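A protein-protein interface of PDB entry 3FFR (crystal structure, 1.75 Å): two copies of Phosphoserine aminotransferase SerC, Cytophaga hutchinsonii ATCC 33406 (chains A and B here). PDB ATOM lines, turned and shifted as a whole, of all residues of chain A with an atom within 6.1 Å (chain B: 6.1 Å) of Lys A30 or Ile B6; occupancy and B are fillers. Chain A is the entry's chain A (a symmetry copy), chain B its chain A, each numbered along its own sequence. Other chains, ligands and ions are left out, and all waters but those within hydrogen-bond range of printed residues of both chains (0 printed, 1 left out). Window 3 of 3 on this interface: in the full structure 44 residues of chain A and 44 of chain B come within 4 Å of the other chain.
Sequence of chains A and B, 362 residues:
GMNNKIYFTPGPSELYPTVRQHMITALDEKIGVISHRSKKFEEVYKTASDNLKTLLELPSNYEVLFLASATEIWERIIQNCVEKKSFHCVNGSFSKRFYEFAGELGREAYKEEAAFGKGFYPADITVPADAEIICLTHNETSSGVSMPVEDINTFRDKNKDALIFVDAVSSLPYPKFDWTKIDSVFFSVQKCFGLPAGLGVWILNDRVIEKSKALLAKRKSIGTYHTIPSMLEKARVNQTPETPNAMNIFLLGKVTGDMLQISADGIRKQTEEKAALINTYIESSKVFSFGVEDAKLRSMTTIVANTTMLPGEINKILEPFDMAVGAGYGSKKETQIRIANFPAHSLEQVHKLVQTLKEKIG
The backbone NH (N) of Asn B3 lies within hydrogen-bond range of the backbone carbonyl oxygen (O) of Asp A28 (2.9 Å). O of Glu A29 sits at hydrogen-bond distance from ND2 of Asn B3. NZ of Lys A30 is in hydrogen-bond range of O of Lys B5 (2.8 Å). The side-chain amino group (NZ) of Lys A30 is in salt-bridge range of the side-chain carboxylate (OE2) of Glu B14, 2.8 Å away.
Of the 10 printed residues of chain A, 4 touch a printed residue of chain B. Printed residues of chain A that touch a printed residue of chain B: Asp A28, Glu A29, Lys A30 and Val A33. Of the 13 printed residues of chain B, 5 touch a printed residue of chain A. Hydrophobic or aromatic side chains of chain B within 4 Å of the printed part of chain A: Ile B6 and Tyr B7.
The side-chain amide oxygen (OD1) of Asn B3 lies within hydrogen-bond range of the backbone NH (N) of Lys B5, at 3.2 Å. The side-chain hydroxyl of Tyr B7 lies within hydrogen-bond range of the side-chain amide nitrogen of Asn B3, 3.1 Å away. N of Ile B6 lies within hydrogen-bond range of O of Asp B322, 2.8 Å away. O of Ile B6 is in hydrogen-bond range of N of Ala B324. The backbone NH (N) of Tyr B7 sits at hydrogen-bond distance from the side-chain carboxylate (OE1) of Glu B14, 3.0 Å away. The backbone carbonyl oxygen (O) of Tyr B7 is in hydrogen-bond range of a ring nitrogen (NE2) of His B345 (2.9 Å).
Lys A30 touches Asn B3 (CE to O, 3.4 Å). NZ of Lys A30 touches CD1 of Ile B6, 3.6 Å away. Val A33 touches Tyr B7 (CG1 to CD1, 3.4 Å). CG1 of Val A33 touches N of Glu B14, 3.8 Å away.
No position is printed for both chains.
Printed residues of chain B within 4 Å of Asp A28: Asn B3 (2.9 Å). Printed residues of chain B within 4 Å of Glu A29: Asn B3. Ile A31 touches none of the printed residues of chain B. Of the printed residues of chain B, Val A33 touches Tyr B7 and Glu B14. Of chain A, only Lys A30 (3.6 Å) comes within 4 Å of Ile B6. Of the printed residues of chain A, Tyr B7 touches Val A33. Phe B8 touches none of the printed residues of chain A. Of the printed residues of chain A, Glu B14 touches Lys A30 and Val A33. The nearest printed residue of chain A that does not touch Ile B6 is Val A33 (6.3 Å).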
ATOM      1  N   THR A  25      20.198 -29.393 -33.684  1.00  0.00           N
ATOM      2  CA  THR A  25      19.782 -29.590 -32.294  1.00  0.00           C
ATOM      3  C   THR A  25      20.850 -29.063 -31.331  1.00  0.00           C
ATOM      4  O   THR A  25      20.545 -28.409 -30.324  1.00  0.00           O
ATOM      5  CB  THR A  25      19.493 -31.053 -31.985  1.00  0.00           C
ATOM      6  OG1 THR A  25      18.452 -31.522 -32.849  1.00  0.00           O
ATOM      7  CG2 THR A  25      19.039 -31.222 -30.560  1.00  0.00           C
ATOM      8  N   ALA A  26      22.110 -29.348 -31.642  1.00  0.00           N
ATOM      9  CA  ALA A  26      23.251 -28.884 -30.806  1.00  0.00           C
ATOM     10  C   ALA A  26      23.253 -27.383 -30.682  1.00  0.00           C
ATOM     11  O   ALA A  26      23.489 -26.817 -29.611  1.00  0.00           O
ATOM     12  CB  ALA A  26      24.636 -29.381 -31.382  1.00  0.00           C
ATOM     13  N   LEU A  27      22.974 -26.726 -31.799  1.00  0.00           N
ATOM     14  CA  LEU A  27      22.994 -25.266 -31.800  1.00  0.00           C
ATOM     15  C   LEU A  27      21.810 -24.756 -30.992  1.00  0.00           C
ATOM     16  O   LEU A  27      21.934 -23.835 -30.168  1.00  0.00           O
ATOM     17  CB  LEU A  27      22.921 -24.722 -33.221  1.00  0.00           C
ATOM     18  CG  LEU A  27      24.143 -24.990 -34.098  1.00  0.00           C
ATOM     19  CD1 LEU A  27      23.834 -24.666 -35.564  1.00  0.00           C
ATOM     20  CD2 LEU A  27      25.419 -24.270 -33.566  1.00  0.00           C
ATOM     21  N   ASP A  28      20.671 -25.374 -31.220  1.00  0.00           N
ATOM     22  CA  ASP A  28      19.429 -24.968 -30.548  1.00  0.00           C
ATOM     23  C   ASP A  28      19.492 -25.104 -29.049  1.00  0.00           C
ATOM     24  O   ASP A  28      18.969 -24.238 -28.299  1.00  0.00           O
ATOM     25  CB  ASP A  28      18.222 -25.779 -31.046  1.00  0.00           C
ATOM     26  CG  ASP A  28      17.720 -25.319 -32.396  1.00  0.00           C
ATOM     27  OD1 ASP A  28      18.107 -24.232 -32.828  1.00  0.00           O
ATOM     28  OD2 ASP A  28      16.895 -26.029 -33.001  1.00  0.00           O
ATOM     29  N   GLU A  29      20.141 -26.178 -28.612  1.00  0.00           N
ATOM     30  CA  GLU A  29      20.266 -26.495 -27.176  1.00  0.00           C
ATOM     31  C   GLU A  29      21.453 -25.832 -26.508  1.00  0.00           C
ATOM     32  O   GLU A  29      21.643 -25.965 -25.301  1.00  0.00           O
ATOM     33  CB  GLU A  29      20.360 -27.990 -26.925  1.00  0.00           C
ATOM     34  CG  GLU A  29      19.059 -28.722 -27.369  1.00  0.00           C
ATOM     35  CD  GLU A  29      19.007 -30.201 -27.006  1.00  0.00           C
ATOM     36  OE1 GLU A  29      19.926 -30.729 -26.357  1.00  0.00           O
ATOM     37  OE2 GLU A  29      18.001 -30.850 -27.380  1.00  0.00           O
ATOM     38  N   LYS A  30      22.241 -25.132 -27.310  1.00  0.00           N
ATOM     39  CA  LYS A  30      23.454 -24.457 -26.826  1.00  0.00           C
ATOM     40  C   LYS A  30      24.466 -25.414 -26.184  1.00  0.00           C
ATOM     41  O   LYS A  30      25.123 -25.104 -25.205  1.00  0.00           O
ATOM     42  CB  LYS A  30      23.114 -23.273 -25.888  1.00  0.00           C
ATOM     43  CG  LYS A  30      22.412 -22.158 -26.660  1.00  0.00           C
ATOM     44  CD  LYS A  30      22.323 -20.883 -25.826  1.00  0.00           C
ATOM     45  CE  LYS A  30      21.863 -19.690 -26.676  1.00  0.00           C
ATOM     46  NZ  LYS A  30      21.850 -18.402 -25.926  1.00  0.00           N
ATOM     47  N   ILE A  31      24.605 -26.574 -26.810  1.00  0.00           N
ATOM     48  CA  ILE A  31      25.530 -27.588 -26.337  1.00  0.00           C
ATOM     49  C   ILE A  31      26.955 -27.040 -26.279  1.00  0.00           C
ATOM     50  O   ILE A  31      27.755 -27.447 -25.445  1.00  0.00           O
ATOM     51  CB  ILE A  31      25.469 -28.881 -27.243  1.00  0.00           C
ATOM     52  CG1 ILE A  31      24.108 -29.551 -27.147  1.00  0.00           C
ATOM     53  CG2 ILE A  31      26.620 -29.867 -26.867  1.00  0.00           C
ATOM     54  CD1 ILE A  31      23.757 -30.061 -25.761  1.00  0.00           C
ATOM     55  N   GLY A  32      27.246 -26.074 -27.146  1.00  0.00           N
ATOM     56  CA  GLY A  32      28.600 -25.490 -27.258  1.00  0.00           C
ATOM     57  C   GLY A  32      28.896 -24.436 -26.197  1.00  0.00           C
ATOM     58  O   GLY A  32      30.043 -23.970 -26.026  1.00  0.00           O
ATOM     59  N   VAL A  33      27.846 -24.124 -25.452  1.00  0.00           N
ATOM     60  CA  VAL A  33      27.852 -23.074 -24.431  1.00  0.00           C
ATOM     61  C   VAL A  33      27.884 -23.616 -23.006  1.00  0.00           C
ATOM     62  O   VAL A  33      28.439 -22.988 -22.099  1.00  0.00           O
ATOM     63  CB  VAL A  33      26.593 -22.148 -24.604  1.00  0.00           C
ATOM     64  CG1 VAL A  33      26.493 -21.077 -23.494  1.00  0.00           C
ATOM     65  CG2 VAL A  33      26.616 -21.474 -26.000  1.00  0.00           C
ATOM     66  N   ILE A  34      27.224 -24.747 -22.808  1.00  0.00           N
ATOM     67  CA  ILE A  34      27.117 -25.336 -21.468  1.00  0.00           C
ATOM     68  C   ILE A  34      28.488 -25.687 -20.907  1.00  0.00           C
ATOM     69  O   ILE A  34      29.445 -25.990 -21.640  1.00  0.00           O
ATOM     70  CB  ILE A  34      26.159 -26.582 -21.409  1.00  0.00           C
ATOM     71  CG1 ILE A  34      26.744 -27.739 -22.238  1.00  0.00           C
ATOM     72  CG2 ILE A  34      24.715 -26.172 -21.836  1.00  0.00           C
ATOM     73  CD1 ILE A  34      25.971 -29.020 -22.205  1.00  0.00           C
ATOM     74  N   ASN B   3      17.017 -23.262 -26.402  1.00  0.00           N
ATOM     75  CA  ASN B   3      17.644 -22.705 -25.187  1.00  0.00           C
ATOM     76  C   ASN B   3      17.877 -21.230 -25.439  1.00  0.00           C
ATOM     77  O   ASN B   3      18.710 -20.853 -26.268  1.00  0.00           O
ATOM     78  CB  ASN B   3      18.946 -23.438 -24.910  1.00  0.00           C
ATOM     79  CG  ASN B   3      19.602 -23.036 -23.595  1.00  0.00           C
ATOM     80  OD1 ASN B   3      19.252 -22.033 -22.959  1.00  0.00           O
ATOM     81  ND2 ASN B   3      20.568 -23.830 -23.187  1.00  0.00           N
ATOM     82  N   ASN B   4      17.127 -20.394 -24.735  1.00  0.00           N
ATOM     83  CA  ASN B   4      17.168 -18.962 -24.949  1.00  0.00           C
ATOM     84  C   ASN B   4      17.968 -18.184 -23.902  1.00  0.00           C
ATOM     85  O   ASN B   4      18.052 -16.969 -23.939  1.00  0.00           O
ATOM     86  CB  ASN B   4      15.745 -18.423 -25.000  1.00  0.00           C
ATOM     87  CG  ASN B   4      14.998 -18.943 -26.209  1.00  0.00           C
ATOM     88  OD1 ASN B   4      15.593 -19.115 -27.279  1.00  0.00           O
ATOM     89  ND2 ASN B   4      13.710 -19.213 -26.049  1.00  0.00           N
ATOM     90  N   LYS B   5      18.545 -18.924 -22.981  1.00  0.00           N
ATOM     91  CA  LYS B   5      19.307 -18.341 -21.901  1.00  0.00           C
ATOM     92  C   LYS B   5      20.654 -17.804 -22.402  1.00  0.00           C
ATOM     93  O   LYS B   5      21.337 -18.449 -23.212  1.00  0.00           O
ATOM     94  CB  LYS B   5      19.532 -19.392 -20.820  1.00  0.00           C
ATOM     95  CG  LYS B   5      20.134 -18.865 -19.566  1.00  0.00           C
ATOM     96  CD  LYS B   5      20.643 -19.993 -18.706  1.00  0.00           C
ATOM     97  CE  LYS B   5      19.564 -20.599 -17.881  1.00  0.00           C
ATOM     98  NZ  LYS B   5      20.043 -21.898 -17.330  1.00  0.00           N
ATOM     99  N   ILE B   6      21.007 -16.611 -21.928  1.00  0.00           N
ATOM    100  CA  ILE B   6      22.298 -15.993 -22.248  1.00  0.00           C
ATOM    101  C   ILE B   6      23.243 -16.303 -21.089  1.00  0.00           C
ATOM    102  O   ILE B   6      22.959 -15.990 -19.924  1.00  0.00           O
ATOM    103  CB  ILE B   6      22.157 -14.476 -22.475  1.00  0.00           C
ATOM    104  CG1 ILE B   6      21.096 -14.225 -23.563  1.00  0.00           C
ATOM    105  CG2 ILE B   6      23.524 -13.812 -22.807  1.00  0.00           C
ATOM    106  CD1 ILE B   6      21.374 -14.933 -24.896  1.00  0.00           C
ATOM    107  N   TYR B   7      24.382 -16.902 -21.436  1.00  0.00           N
ATOM    108  CA  TYR B   7      25.337 -17.365 -20.440  1.00  0.00           C
ATOM    109  C   TYR B   7      26.541 -16.440 -20.277  1.00  0.00           C
ATOM    110  O   TYR B   7      27.356 -16.336 -21.178  1.00  0.00           O
ATOM    111  CB  TYR B   7      25.842 -18.771 -20.852  1.00  0.00           C
ATOM    112  CG  TYR B   7      24.827 -19.880 -20.791  1.00  0.00           C
ATOM    113  CD1 TYR B   7      23.821 -19.994 -21.743  1.00  0.00           C
ATOM    114  CD2 TYR B   7      24.901 -20.845 -19.805  1.00  0.00           C
ATOM    115  CE1 TYR B   7      22.910 -21.012 -21.689  1.00  0.00           C
ATOM    116  CE2 TYR B   7      24.001 -21.867 -19.748  1.00  0.00           C
ATOM    117  CZ  TYR B   7      23.003 -21.956 -20.686  1.00  0.00           C
ATOM    118  OH  TYR B   7      22.109 -22.994 -20.617  1.00  0.00           O
ATOM    119  N   PHE B   8      26.641 -15.806 -19.106  1.00  0.00           N
ATOM    120  CA  PHE B   8      27.793 -14.982 -18.786  1.00  0.00           C
ATOM    121  C   PHE B   8      28.764 -15.816 -17.960  1.00  0.00           C
ATOM    122  O   PHE B   8      29.308 -15.376 -16.942  1.00  0.00           O
ATOM    123  CB  PHE B   8      27.368 -13.723 -18.018  1.00  0.00           C
ATOM    124  CG  PHE B   8      26.427 -12.834 -18.798  1.00  0.00           C
ATOM    125  CD1 PHE B   8      26.912 -11.824 -19.614  1.00  0.00           C
ATOM    126  CD2 PHE B   8      25.055 -13.010 -18.700  1.00  0.00           C
ATOM    127  CE1 PHE B   8      26.069 -10.992 -20.309  1.00  0.00           C
ATOM    128  CE2 PHE B   8      24.190 -12.197 -19.395  1.00  0.00           C
ATOM    129  CZ  PHE B   8      24.699 -11.173 -20.214  1.00  0.00           C
ATOM    130  N   GLU B  14      28.769 -18.046 -24.084  1.00  0.00           N
ATOM    131  CA  GLU B  14      27.894 -17.679 -25.176  1.00  0.00           C
ATOM    132  C   GLU B  14      28.699 -17.681 -26.503  1.00  0.00           C
ATOM    133  O   GLU B  14      29.794 -17.127 -26.585  1.00  0.00           O
ATOM    134  CB  GLU B  14      27.271 -16.307 -24.890  1.00  0.00           C
ATOM    135  CG  GLU B  14      26.077 -15.926 -25.695  1.00  0.00           C
ATOM    136  CD  GLU B  14      24.850 -16.807 -25.479  1.00  0.00           C
ATOM    137  OE1 GLU B  14      24.647 -17.449 -24.411  1.00  0.00           O
ATOM    138  OE2 GLU B  14      24.059 -16.822 -26.424  1.00  0.00           O
ATOM    139  N   ASP B 322      16.107 -15.112 -18.678  1.00  0.00           N
ATOM    140  CA  ASP B 322      16.969 -15.763 -19.678  1.00  0.00           C
ATOM    141  C   ASP B 322      18.431 -15.337 -19.640  1.00  0.00           C
ATOM    142  O   ASP B 322      19.046 -14.995 -20.667  1.00  0.00           O
ATOM    143  CB  ASP B 322      16.420 -15.532 -21.075  1.00  0.00           C
ATOM    144  CG  ASP B 322      15.343 -16.537 -21.435  1.00  0.00           C
ATOM    145  OD1 ASP B 322      15.455 -17.725 -21.024  1.00  0.00           O
ATOM    146  OD2 ASP B 322      14.419 -16.131 -22.154  1.00  0.00           O
ATOM    147  N   MET B 323      18.962 -15.357 -18.430  1.00  0.00           N
ATOM    148  CA  MET B 323      20.385 -15.072 -18.192  1.00  0.00           C
ATOM    149  C   MET B 323      20.929 -15.933 -17.064  1.00  0.00           C
ATOM    150  O   MET B 323      20.188 -16.429 -16.213  1.00  0.00           O
ATOM    151  CB  MET B 323      20.609 -13.597 -17.845  1.00  0.00           C
ATOM    152  CG  MET B 323      20.196 -12.641 -18.971  1.00  0.00           C
ATOM    153  SD  MET B 323      20.521 -10.786 -18.566  1.00  0.00           S
ATOM    154  CE  MET B 323      19.157 -10.542 -17.204  1.00  0.00           C
ATOM    155  N   ALA B 324      22.238 -16.132 -17.104  1.00  0.00           N
ATOM    156  CA  ALA B 324      22.955 -16.837 -16.034  1.00  0.00           C
ATOM    157  C   ALA B 324      24.379 -16.310 -15.930  1.00  0.00           C
ATOM    158  O   ALA B 324      24.964 -15.911 -16.924  1.00  0.00           O
ATOM    159  CB  ALA B 324      22.975 -18.352 -16.273  1.00  0.00           C
ATOM    160  N   VAL B 325      24.886 -16.278 -14.707  1.00  0.00           N
ATOM    161  CA  VAL B 325      26.280 -15.907 -14.423  1.00  0.00           C
ATOM    162  C   VAL B 325      26.988 -17.144 -13.866  1.00  0.00           C
ATOM    163  O   VAL B 325      26.358 -18.111 -13.449  1.00  0.00           O
ATOM    164  CB  VAL B 325      26.390 -14.728 -13.428  1.00  0.00           C
ATOM    165  CG1 VAL B 325      25.614 -13.537 -13.973  1.00  0.00           C
ATOM    166  CG2 VAL B 325      25.915 -15.109 -12.037  1.00  0.00           C
ATOM    167  N   HIS B 345      29.300 -11.271 -25.910  1.00  0.00           N
ATOM    168  CA  HIS B 345      28.303 -10.577 -25.067  1.00  0.00           C
ATOM    169  C   HIS B 345      28.179  -9.140 -25.536  1.00  0.00           C
ATOM    170  O   HIS B 345      29.161  -8.414 -25.602  1.00  0.00           O
ATOM    171  CB  HIS B 345      28.730 -10.611 -23.592  1.00  0.00           C
ATOM    172  CG  HIS B 345      28.934 -11.999 -23.067  1.00  0.00           C
ATOM    173  ND1 HIS B 345      30.180 -12.518 -22.791  1.00  0.00           N
ATOM    174  CD2 HIS B 345      28.043 -12.984 -22.787  1.00  0.00           C
ATOM    175  CE1 HIS B 345      30.048 -13.774 -22.387  1.00  0.00           C
ATOM    176  NE2 HIS B 345      28.763 -14.079 -22.376  1.00  0.00           N
ATOM    177  N   GLN B 349      23.091  -6.807 -23.932  1.00  0.00           N
ATOM    178  CA  GLN B 349      22.958  -7.980 -23.058  1.00  0.00           C
ATOM    179  C   GLN B 349      23.487  -7.659 -21.643  1.00  0.00           C
ATOM    180  O   GLN B 349      22.859  -7.987 -20.638  1.00  0.00           O
ATOM    181  CB  GLN B 349      23.690  -9.191 -23.637  1.00  0.00           C
ATOM    182  CG  GLN B 349      22.954  -9.810 -24.837  1.00  0.00           C
ATOM    183  CD  GLN B 349      23.772 -10.859 -25.574  1.00  0.00           C
ATOM    184  OE1 GLN B 349      24.991 -10.759 -25.642  1.00  0.00           O
ATOM    185  NE2 GLN B 349      23.088 -11.847 -26.180  1.00  0.00           N
